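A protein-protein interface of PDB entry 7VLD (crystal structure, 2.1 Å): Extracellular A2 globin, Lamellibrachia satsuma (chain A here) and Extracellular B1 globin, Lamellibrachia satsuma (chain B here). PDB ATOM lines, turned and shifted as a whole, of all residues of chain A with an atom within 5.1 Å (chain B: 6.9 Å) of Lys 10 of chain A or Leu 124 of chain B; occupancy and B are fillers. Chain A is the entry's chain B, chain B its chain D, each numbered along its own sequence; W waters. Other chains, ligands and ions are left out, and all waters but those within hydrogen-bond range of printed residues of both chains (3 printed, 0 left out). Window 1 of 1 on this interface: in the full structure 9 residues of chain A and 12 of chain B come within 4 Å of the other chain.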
ATOM      1  N   LEU A   6      23.330  24.158 -28.531  1.00  0.00           N
ATOM      2  CA  LEU A   6      22.777  24.342 -27.192  1.00  0.00           C
ATOM      3  C   LEU A   6      23.554  23.538 -26.157  1.00  0.00           C
ATOM      4  O   LEU A   6      23.800  24.021 -25.045  1.00  0.00           O
ATOM      5  CB  LEU A   6      21.299  23.948 -27.172  1.00  0.00           C
ATOM      6  CG  LEU A   6      20.357  24.698 -28.117  1.00  0.00           C
ATOM      7  CD1 LEU A   6      18.958  24.104 -28.055  1.00  0.00           C
ATOM      8  CD2 LEU A   6      20.326  26.181 -27.787  1.00  0.00           C
ATOM      9  N   GLN A   7      23.943  22.307 -26.501  1.00  0.00           N
ATOM     10  CA  GLN A   7      24.715  21.491 -25.569  1.00  0.00           C
ATOM     11  C   GLN A   7      26.076  22.112 -25.288  1.00  0.00           C
ATOM     12  O   GLN A   7      26.576  22.038 -24.160  1.00  0.00           O
ATOM     13  CB  GLN A   7      24.878  20.072 -26.114  1.00  0.00           C
ATOM     14  CG  GLN A   7      23.621  19.221 -26.042  1.00  0.00           C
ATOM     15  CD  GLN A   7      22.587  19.605 -27.081  1.00  0.00           C
ATOM     16  OE1 GLN A   7      22.926  20.014 -28.191  1.00  0.00           O
ATOM     17  NE2 GLN A   7      21.314  19.480 -26.722  1.00  0.00           N
ATOM     18  N   ARG A   8      26.687  22.729 -26.301  1.00  0.00           N
ATOM     19  CA  ARG A   8      27.982  23.370 -26.102  1.00  0.00           C
ATOM     20  C   ARG A   8      27.875  24.545 -25.138  1.00  0.00           C
ATOM     21  O   ARG A   8      28.747  24.732 -24.282  1.00  0.00           O
ATOM     22  CB  ARG A   8      28.553  23.807 -27.451  1.00  0.00           C
ATOM     23  CG  ARG A   8      28.949  22.630 -28.330  1.00  0.00           C
ATOM     24  CD  ARG A   8      29.084  22.990 -29.801  1.00  0.00           C
ATOM     25  NE  ARG A   8      29.186  21.784 -30.620  1.00  0.00           N
ATOM     26  CZ  ARG A   8      30.323  21.298 -31.111  1.00  0.00           C
ATOM     27  NH1 ARG A   8      31.471  21.920 -30.883  1.00  0.00           N
ATOM     28  NH2 ARG A   8      30.309  20.190 -31.840  1.00  0.00           N
ATOM     29  N   LEU A   9      26.803  25.336 -25.248  1.00  0.00           N
ATOM     30  CA  LEU A   9      26.596  26.436 -24.310  1.00  0.00           C
ATOM     31  C   LEU A   9      26.408  25.923 -22.889  1.00  0.00           C
ATOM     32  O   LEU A   9      26.957  26.490 -21.937  1.00  0.00           O
ATOM     33  CB  LEU A   9      25.389  27.271 -24.734  1.00  0.00           C
ATOM     34  CG  LEU A   9      25.448  27.940 -26.105  1.00  0.00           C
ATOM     35  CD1 LEU A   9      24.201  28.780 -26.341  1.00  0.00           C
ATOM     36  CD2 LEU A   9      26.703  28.787 -26.230  1.00  0.00           C
ATOM     37  N   LYS A  10      25.632  24.851 -22.726  1.00  0.00           N
ATOM     38  CA  LYS A  10      25.390  24.300 -21.397  1.00  0.00           C
ATOM     39  C   LYS A  10      26.670  23.746 -20.787  1.00  0.00           C
ATOM     40  O   LYS A  10      26.967  23.991 -19.611  1.00  0.00           O
ATOM     41  CB  LYS A  10      24.324  23.212 -21.472  1.00  0.00           C
ATOM     42  CG  LYS A  10      23.951  22.628 -20.130  1.00  0.00           C
ATOM     43  CD  LYS A  10      22.596  23.133 -19.695  1.00  0.00           C
ATOM     44  CE  LYS A  10      21.881  22.079 -18.883  1.00  0.00           C
ATOM     45  NZ  LYS A  10      20.407  22.277 -18.883  1.00  0.00           N
ATOM     46  N   VAL A  11      27.436  22.983 -21.572  1.00  0.00           N
ATOM     47  CA  VAL A  11      28.693  22.429 -21.082  1.00  0.00           C
ATOM     48  C   VAL A  11      29.667  23.542 -20.720  1.00  0.00           C
ATOM     49  O   VAL A  11      30.427  23.419 -19.753  1.00  0.00           O
ATOM     50  CB  VAL A  11      29.287  21.462 -22.128  1.00  0.00           C
ATOM     51  CG1 VAL A  11      30.713  21.076 -21.774  1.00  0.00           C
ATOM     52  CG2 VAL A  11      28.417  20.217 -22.246  1.00  0.00           C
ATOM     53  N   LYS A  12      29.645  24.649 -21.466  1.00  0.00           N
ATOM     54  CA  LYS A  12      30.514  25.780 -21.153  1.00  0.00           C
ATOM     55  C   LYS A  12      30.197  26.359 -19.780  1.00  0.00           C
ATOM     56  O   LYS A  12      31.095  26.561 -18.955  1.00  0.00           O
ATOM     57  CB  LYS A  12      30.373  26.859 -22.228  1.00  0.00           C
ATOM     58  CG  LYS A  12      31.176  26.611 -23.491  1.00  0.00           C
ATOM     59  CD  LYS A  12      30.650  27.474 -24.625  1.00  0.00           C
ATOM     60  CE  LYS A  12      31.604  27.496 -25.804  1.00  0.00           C
ATOM     61  NZ  LYS A  12      32.832  28.281 -25.501  1.00  0.00           N
ATOM     62  N   ARG A  13      28.918  26.638 -19.519  1.00  0.00           N
ATOM     63  CA  ARG A  13      28.539  27.251 -18.250  1.00  0.00           C
ATOM     64  C   ARG A  13      28.765  26.297 -17.084  1.00  0.00           C
ATOM     65  O   ARG A  13      29.276  26.706 -16.033  1.00  0.00           O
ATOM     66  CB  ARG A  13      27.080  27.705 -18.305  1.00  0.00           C
ATOM     67  CG  ARG A  13      26.606  28.430 -17.058  1.00  0.00           C
ATOM     68  CD  ARG A  13      25.161  28.875 -17.203  1.00  0.00           C
ATOM     69  NE  ARG A  13      24.297  27.775 -17.624  1.00  0.00           N
ATOM     70  CZ  ARG A  13      23.777  26.875 -16.796  1.00  0.00           C
ATOM     71  NH1 ARG A  13      23.003  25.909 -17.267  1.00  0.00           N
ATOM     72  NH2 ARG A  13      24.036  26.939 -15.497  1.00  0.00           N
ATOM     73  N   GLN A  14      28.402  25.023 -17.247  1.00  0.00           N
ATOM     74  CA  GLN A  14      28.603  24.062 -16.166  1.00  0.00           C
ATOM     75  C   GLN A  14      30.085  23.819 -15.906  1.00  0.00           C
ATOM     76  O   GLN A  14      30.496  23.642 -14.752  1.00  0.00           O
ATOM     77  CB  GLN A  14      27.882  22.751 -16.479  1.00  0.00           C
ATOM     78  CG  GLN A  14      26.366  22.857 -16.422  1.00  0.00           C
ATOM     79  CD  GLN A  14      25.688  21.506 -16.299  1.00  0.00           C
ATOM     80  OE1 GLN A  14      26.305  20.464 -16.526  1.00  0.00           O
ATOM     81  NE2 GLN A  14      24.413  21.516 -15.926  1.00  0.00           N
ATOM     82  N   TRP A  15      30.907  23.809 -16.961  1.00  0.00           N
ATOM     83  CA  TRP A  15      32.348  23.674 -16.764  1.00  0.00           C
ATOM     84  C   TRP A  15      32.911  24.878 -16.020  1.00  0.00           C
ATOM     85  O   TRP A  15      33.704  24.728 -15.084  1.00  0.00           O
ATOM     86  CB  TRP A  15      33.063  23.499 -18.103  1.00  0.00           C
ATOM     87  CG  TRP A  15      34.554  23.659 -17.992  1.00  0.00           C
ATOM     88  CD1 TRP A  15      35.286  24.772 -18.296  1.00  0.00           C
ATOM     89  CD2 TRP A  15      35.491  22.680 -17.525  1.00  0.00           C
ATOM     90  NE1 TRP A  15      36.618  24.543 -18.055  1.00  0.00           N
ATOM     91  CE2 TRP A  15      36.772  23.267 -17.581  1.00  0.00           C
ATOM     92  CE3 TRP A  15      35.372  21.363 -17.069  1.00  0.00           C
ATOM     93  CZ2 TRP A  15      37.925  22.582 -17.198  1.00  0.00           C
ATOM     94  CZ3 TRP A  15      36.518  20.686 -16.689  1.00  0.00           C
ATOM     95  CH2 TRP A  15      37.777  21.297 -16.757  1.00  0.00           C
ATOM     96  N   VAL A 124      21.658  19.374 -11.186  1.00  0.00           N
ATOM     97  CA  VAL A 124      21.738  20.147 -12.422  1.00  0.00           C
ATOM     98  C   VAL A 124      22.613  19.499 -13.483  1.00  0.00           C
ATOM     99  O   VAL A 124      22.578  19.946 -14.641  1.00  0.00           O
ATOM    100  CB  VAL A 124      22.226  21.587 -12.154  1.00  0.00           C
ATOM    101  CG1 VAL A 124      21.300  22.293 -11.176  1.00  0.00           C
ATOM    102  CG2 VAL A 124      23.655  21.574 -11.636  1.00  0.00           C
ATOM    103  N   ASP A 126      24.031  17.796 -16.503  1.00  0.00           N
ATOM    104  CA  ASP A 126      23.445  17.380 -17.778  1.00  0.00           C
ATOM    105  C   ASP A 126      24.342  16.288 -18.352  1.00  0.00           C
ATOM    106  O   ASP A 126      25.330  16.563 -19.033  1.00  0.00           O
ATOM    107  CB  ASP A 126      23.313  18.573 -18.722  1.00  0.00           C
ATOM    108  CG  ASP A 126      22.448  18.276 -19.938  1.00  0.00           C
ATOM    109  OD1 ASP A 126      22.469  17.130 -20.436  1.00  0.00           O
ATOM    110  OD2 ASP A 126      21.748  19.200 -20.402  1.00  0.00           O
ATOM    111  N   ALA A 129      24.496  16.091 -22.384  1.00  0.00           N
ATOM    112  CA  ALA A 129      25.310  17.141 -22.989  1.00  0.00           C
ATOM    113  C   ALA A 129      26.793  16.899 -22.745  1.00  0.00           C
ATOM    114  O   ALA A 129      27.620  17.103 -23.642  1.00  0.00           O
ATOM    115  CB  ALA A 129      24.894  18.509 -22.447  1.00  0.00           C
ATOM    116  N   GLN B  15      16.427  32.137 -13.673  1.00  0.00           N
ATOM    117  CA  GLN B  15      16.798  31.139 -14.671  1.00  0.00           C
ATOM    118  C   GLN B  15      17.131  31.780 -16.012  1.00  0.00           C
ATOM    119  O   GLN B  15      18.009  31.288 -16.729  1.00  0.00           O
ATOM    120  CB  GLN B  15      15.678  30.109 -14.829  1.00  0.00           C
ATOM    121  CG  GLN B  15      15.488  29.224 -13.606  1.00  0.00           C
ATOM    122  CD  GLN B  15      14.583  28.036 -13.871  1.00  0.00           C
ATOM    123  OE1 GLN B  15      13.829  28.018 -14.845  1.00  0.00           O
ATOM    124  NE2 GLN B  15      14.657  27.033 -13.005  1.00  0.00           N
ATOM    125  N   GLN B  18      20.652  33.157 -16.015  1.00  0.00           N
ATOM    126  CA  GLN B  18      21.676  32.128 -16.178  1.00  0.00           C
ATOM    127  C   GLN B  18      22.287  32.174 -17.572  1.00  0.00           C
ATOM    128  O   GLN B  18      23.508  32.068 -17.729  1.00  0.00           O
ATOM    129  CB  GLN B  18      21.085  30.738 -15.933  1.00  0.00           C
ATOM    130  CG  GLN B  18      20.855  30.347 -14.488  1.00  0.00           C
ATOM    131  CD  GLN B  18      20.321  28.929 -14.368  1.00  0.00           C
ATOM    132  OE1 GLN B  18      20.702  28.043 -15.135  1.00  0.00           O
ATOM    133  NE2 GLN B  18      19.425  28.712 -13.413  1.00  0.00           N
ATOM    134  N   ILE B  19      21.449  32.323 -18.596  1.00  0.00           N
ATOM    135  CA  ILE B  19      21.879  32.186 -19.982  1.00  0.00           C
ATOM    136  C   ILE B  19      21.881  33.504 -20.739  1.00  0.00           C
ATOM    137  O   ILE B  19      22.379  33.545 -21.876  1.00  0.00           O
ATOM    138  CB  ILE B  19      21.014  31.154 -20.736  1.00  0.00           C
ATOM    139  CG1 ILE B  19      19.557  31.617 -20.773  1.00  0.00           C
ATOM    140  CG2 ILE B  19      21.115  29.792 -20.069  1.00  0.00           C
ATOM    141  CD1 ILE B  19      18.643  30.707 -21.560  1.00  0.00           C
ATOM    142  N   MET B  32      21.655  31.192 -29.730  1.00  0.00           N
ATOM    143  CA  MET B  32      20.322  30.923 -29.204  1.00  0.00           C
ATOM    144  C   MET B  32      19.249  31.468 -30.137  1.00  0.00           C
ATOM    145  O   MET B  32      18.240  30.800 -30.393  1.00  0.00           O
ATOM    146  CB  MET B  32      20.176  31.531 -27.808  1.00  0.00           C
ATOM    147  CG  MET B  32      21.100  30.928 -26.761  1.00  0.00           C
ATOM    148  SD  MET B  32      20.993  31.784 -25.176  1.00  0.00           S
ATOM    149  CE  MET B  32      19.217  31.918 -24.986  1.00  0.00           C
ATOM    150  N   ILE B  36      16.352  29.255 -32.005  1.00  0.00           N
ATOM    151  CA  ILE B  36      14.938  29.530 -31.768  1.00  0.00           C
ATOM    152  C   ILE B  36      14.199  29.713 -33.087  1.00  0.00           C
ATOM    153  O   ILE B  36      13.132  29.128 -33.306  1.00  0.00           O
ATOM    154  CB  ILE B  36      14.781  30.758 -30.855  1.00  0.00           C
ATOM    155  CG1 ILE B  36      15.229  30.423 -29.430  1.00  0.00           C
ATOM    156  CG2 ILE B  36      13.343  31.251 -30.866  1.00  0.00           C
ATOM    157  CD1 ILE B  36      15.193  31.601 -28.486  1.00  0.00           C
ATOM    158  N   THR B 119      10.791  24.319 -25.515  1.00  0.00           N
ATOM    159  CA  THR B 119      11.636  23.204 -25.927  1.00  0.00           C
ATOM    160  C   THR B 119      13.121  23.537 -25.826  1.00  0.00           C
ATOM    161  O   THR B 119      13.911  22.705 -25.364  1.00  0.00           O
ATOM    162  CB  THR B 119      11.291  22.788 -27.362  1.00  0.00           C
ATOM    163  OG1 THR B 119       9.908  22.420 -27.436  1.00  0.00           O
ATOM    164  CG2 THR B 119      12.147  21.608 -27.802  1.00  0.00           C
ATOM    165  N   VAL B 120      13.513  24.745 -26.231  1.00  0.00           N
ATOM    166  CA  VAL B 120      14.928  25.098 -26.293  1.00  0.00           C
ATOM    167  C   VAL B 120      15.476  25.440 -24.911  1.00  0.00           C
ATOM    168  O   VAL B 120      16.588  25.033 -24.557  1.00  0.00           O
ATOM    169  CB  VAL B 120      15.136  26.255 -27.287  1.00  0.00           C
ATOM    170  CG1 VAL B 120      16.555  26.798 -27.192  1.00  0.00           C
ATOM    171  CG2 VAL B 120      14.833  25.795 -28.704  1.00  0.00           C
ATOM    172  N   LEU B 121      14.712  26.189 -24.116  1.00  0.00           N
ATOM    173  CA  LEU B 121      15.232  26.680 -22.839  1.00  0.00           C
ATOM    174  C   LEU B 121      15.689  25.584 -21.883  1.00  0.00           C
ATOM    175  O   LEU B 121      16.749  25.770 -21.250  1.00  0.00           O
ATOM    176  CB  LEU B 121      14.183  27.579 -22.173  1.00  0.00           C
ATOM    177  CG  LEU B 121      13.962  28.922 -22.870  1.00  0.00           C
ATOM    178  CD1 LEU B 121      12.897  29.732 -22.155  1.00  0.00           C
ATOM    179  CD2 LEU B 121      15.266  29.700 -22.957  1.00  0.00           C
ATOM    180  N   PRO B 122      14.988  24.459 -21.706  1.00  0.00           N
ATOM    181  CA  PRO B 122      15.519  23.414 -20.814  1.00  0.00           C
ATOM    182  C   PRO B 122      16.870  22.870 -21.247  1.00  0.00           C
ATOM    183  O   PRO B 122      17.625  22.372 -20.401  1.00  0.00           O
ATOM    184  CB  PRO B 122      14.433  22.328 -20.850  1.00  0.00           C
ATOM    185  CG  PRO B 122      13.611  22.630 -22.055  1.00  0.00           C
ATOM    186  CD  PRO B 122      13.633  24.116 -22.179  1.00  0.00           C
ATOM    187  N   SER B 123      17.202  22.946 -22.538  1.00  0.00           N
ATOM    188  CA  SER B 123      18.526  22.538 -22.992  1.00  0.00           C
ATOM    189  C   SER B 123      19.620  23.497 -22.544  1.00  0.00           C
ATOM    190  O   SER B 123      20.801  23.137 -22.613  1.00  0.00           O
ATOM    191  CB  SER B 123      18.549  22.418 -24.518  1.00  0.00           C
ATOM    192  OG  SER B 123      17.515  21.570 -24.984  1.00  0.00           O
ATOM    193  N   LEU B 124      19.261  24.696 -22.089  1.00  0.00           N
ATOM    194  CA  LEU B 124      20.226  25.718 -21.706  1.00  0.00           C
ATOM    195  C   LEU B 124      20.234  26.034 -20.221  1.00  0.00           C
ATOM    196  O   LEU B 124      21.268  26.463 -19.701  1.00  0.00           O
ATOM    197  CB  LEU B 124      19.953  27.016 -22.476  1.00  0.00           C
ATOM    198  CG  LEU B 124      20.128  26.982 -23.993  1.00  0.00           C
ATOM    199  CD1 LEU B 124      19.543  28.234 -24.623  1.00  0.00           C
ATOM    200  CD2 LEU B 124      21.598  26.840 -24.348  1.00  0.00           C
ATOM    201  N   ILE B 125      19.118  25.828 -19.527  1.00  0.00           N
ATOM    202  CA  ILE B 125      18.917  26.317 -18.168  1.00  0.00           C
ATOM    203  C   ILE B 125      19.005  25.152 -17.191  1.00  0.00           C
ATOM    204  O   ILE B 125      18.468  24.068 -17.449  1.00  0.00           O
ATOM    205  CB  ILE B 125      17.562  27.044 -18.051  1.00  0.00           C
ATOM    206  CG1 ILE B 125      17.602  28.365 -18.828  1.00  0.00           C
ATOM    207  CG2 ILE B 125      17.178  27.270 -16.595  1.00  0.00           C
ATOM    208  CD1 ILE B 125      16.259  29.059 -18.937  1.00  0.00           C
ATOM    209  N   ASP B 126      19.695  25.375 -16.071  1.00  0.00           N
ATOM    210  CA  ASP B 126      19.728  24.392 -14.996  1.00  0.00           C
ATOM    211  C   ASP B 126      18.381  24.345 -14.287  1.00  0.00           C
ATOM    212  O   ASP B 126      17.871  25.377 -13.838  1.00  0.00           O
ATOM    213  CB  ASP B 126      20.824  24.733 -13.985  1.00  0.00           C
ATOM    214  CG  ASP B 126      22.216  24.529 -14.538  1.00  0.00           C
ATOM    215  OD1 ASP B 126      22.358  23.842 -15.570  1.00  0.00           O
ATOM    216  OD2 ASP B 126      23.172  25.053 -13.930  1.00  0.00           O
ATOM    217  N   ASN B 127      17.814  23.143 -14.175  1.00  0.00           N
ATOM    218  CA  ASN B 127      16.552  22.928 -13.464  1.00  0.00           C
ATOM    219  C   ASN B 127      15.438  23.805 -14.031  1.00  0.00           C
ATOM    220  O   ASN B 127      14.770  24.541 -13.300  1.00  0.00           O
ATOM    221  CB  ASN B 127      16.712  23.178 -11.963  1.00  0.00           C
ATOM    222  CG  ASN B 127      17.152  21.949 -11.212  1.00  0.00           C
ATOM    223  OD1 ASN B 127      18.007  22.024 -10.334  1.00  0.00           O
ATOM    224  ND2 ASN B 127      16.566  20.806 -11.547  1.00  0.00           N
ATOM    225  N   PHE B 128      15.250  23.732 -15.346  1.00  0.00           N
ATOM    226  CA  PHE B 128      14.195  24.509 -15.982  1.00  0.00           C
ATOM    227  C   PHE B 128      12.855  24.198 -15.329  1.00  0.00           C
ATOM    228  O   PHE B 128      12.493  23.032 -15.151  1.00  0.00           O
ATOM    229  CB  PHE B 128      14.141  24.212 -17.481  1.00  0.00           C
ATOM    230  CG  PHE B 128      13.084  24.990 -18.216  1.00  0.00           C
ATOM    231  CD1 PHE B 128      13.266  26.335 -18.501  1.00  0.00           C
ATOM    232  CD2 PHE B 128      11.915  24.375 -18.631  1.00  0.00           C
ATOM    233  CE1 PHE B 128      12.297  27.052 -19.178  1.00  0.00           C
ATOM    234  CE2 PHE B 128      10.943  25.088 -19.310  1.00  0.00           C
ATOM    235  CZ  PHE B 128      11.134  26.428 -19.583  1.00  0.00           C
HETATM  236  O   HOH W   1      23.862  27.303 -20.649  1.00  0.00           O
HETATM  237  O   HOH W   2      21.624  20.427 -23.232  1.00  0.00           O
HETATM  238  O   HOH W   3      20.488  21.300 -16.260  1.00  0.00           O
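Leu 124 of chain B touches four residues of chain A. Of the printed residues of chain A, Ile 125 of chain B touches Lys 10. Of the printed residues of chain B, Arg 13 of chain A touches Gln 18, Leu 124 and Asp 126. Of the printed residues of chain B, Leu 6 of chain A touches Val 120 (3.7 Å), Ser 123 (3.9 Å) and Leu 124 (3.6 Å). Leu 121 of chain B touches none of the printed residues of chain A. Gln 7 of chain A touches none of the printed residues of chain B. The nearest residue of chain B that does not touch Lys 10 of chain A is Asn 127 of chain B (5.4 Å). The nearest printed residue of chain A that does not touch Leu 124 of chain B is Gln 7 of chain A (5.5 Å).
Among the printed residues, merely in contact across the chains: Leu 6 of chain A with Val 120 of chain B (3.7 Å), Leu 6 of chain A with Ser 123 of chain B (3.9 Å), Leu 6 of chain A with Leu 124 of chain B (3.6 Å), Leu 9 of chain A with Met 32 of chain B (3.8 Å), Leu 9 of chain A with Leu 124 of chain B (3.8 Å), Lys 10 of chain A with Ser 123 of chain B (3.4 Å), Lys 10 of chain A with Leu 124 of chain B (3.6 Å), Lys 10 of chain A with Asp 126 of chain B (3.8 Å), Arg 13 of chain A with Gln 18 of chain B (3.5 Å), Val 124 of chain A with Asp 126 of chain B (3.8 Å) and Val 124 of chain A with Asn 127 of chain B (3.4 Å).
O of Pro 122 of chain B sits at hydrogen-bond distance from NZ of Lys 10 of chain A (3.2 Å). The side-chain amino group (NZ) of Lys 10 of chain A sits at hydrogen-bond distance from the backbone carbonyl oxygen (O) of Ile 125 of chain B, at 3.0 Å. NH1 of Arg 13 of chain A sits at hydrogen-bond distance from O of Leu 124 of chain B (3.0 Å). The guanidinium group (NH2) of Arg 13 of chain A is in salt-bridge range of the side-chain carboxylate (OD2) of Asp 126 of chain B (2.6 Å). The side-chain amide nitrogen (NE2) of Gln 14 of chain A is in hydrogen-bond range of the side-chain carboxylate (OD1) of Asp 126 of chain B, 3.1 Å away.
Water W3 lies within hydrogen-bond range of the side-chain amino group (NZ) of Lys 10 of chain A (2.8 Å), the backbone carbonyl oxygen (O) of Val 124 of chain A (3.0 Å) and the side-chain carboxylate (OD1) of Asp 126 of chain B (3.2 Å). Water W1 lies within hydrogen-bond range of the backbone carbonyl oxygen of Leu 124 of chain B (2.9 Å), the guanidinium group of Arg 13 of chain A (3.1 Å) and the backbone carbonyl oxygen of Leu 9 of chain A (3.4 Å). Water W2 bridges the backbone carbonyl oxygen of Ser 123 of chain B (2.9 Å) and the side-chain carboxylate of Asp 126 of chain A (3.1 Å).
Hydrophobic or aromatic side chains of chain A that line the printed part of chain B: Leu 6, Leu 9 and Val 124. Printed residues of chain B that touch a printed residue of chain A: Gln 18, Met 32, Val 120, Pro 122, Ser 123, Leu 124, Ile 125, Asp 126 and Asn 127. Among the printed residues, 16 pairs touch across the chains. Among the printed residues, Asp or Glu carboxylates within 4 Å of a Lys or Arg side-chain nitrogen of the other chain: Arg 13 of chain A with Asp 126 of chain B (2.6 Å).
NZ of Lys 10 of chain A lies within salt-bridge range of OD2 of Asp 126 of chain A (3.7 Å). NE2 of Gln 14 of chain A lies within hydrogen-bond range of O of Val 124 of chain A (2.7 Å). NE2 of Gln 15 of chain B lies within hydrogen-bond range of O of Asn 127 of chain B (2.5 Å). The side-chain amide oxygen (OE1) of Gln 18 of chain B is in hydrogen-bond range of the backbone NH (N) of Asp 126 of chain B (3.0 Å).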
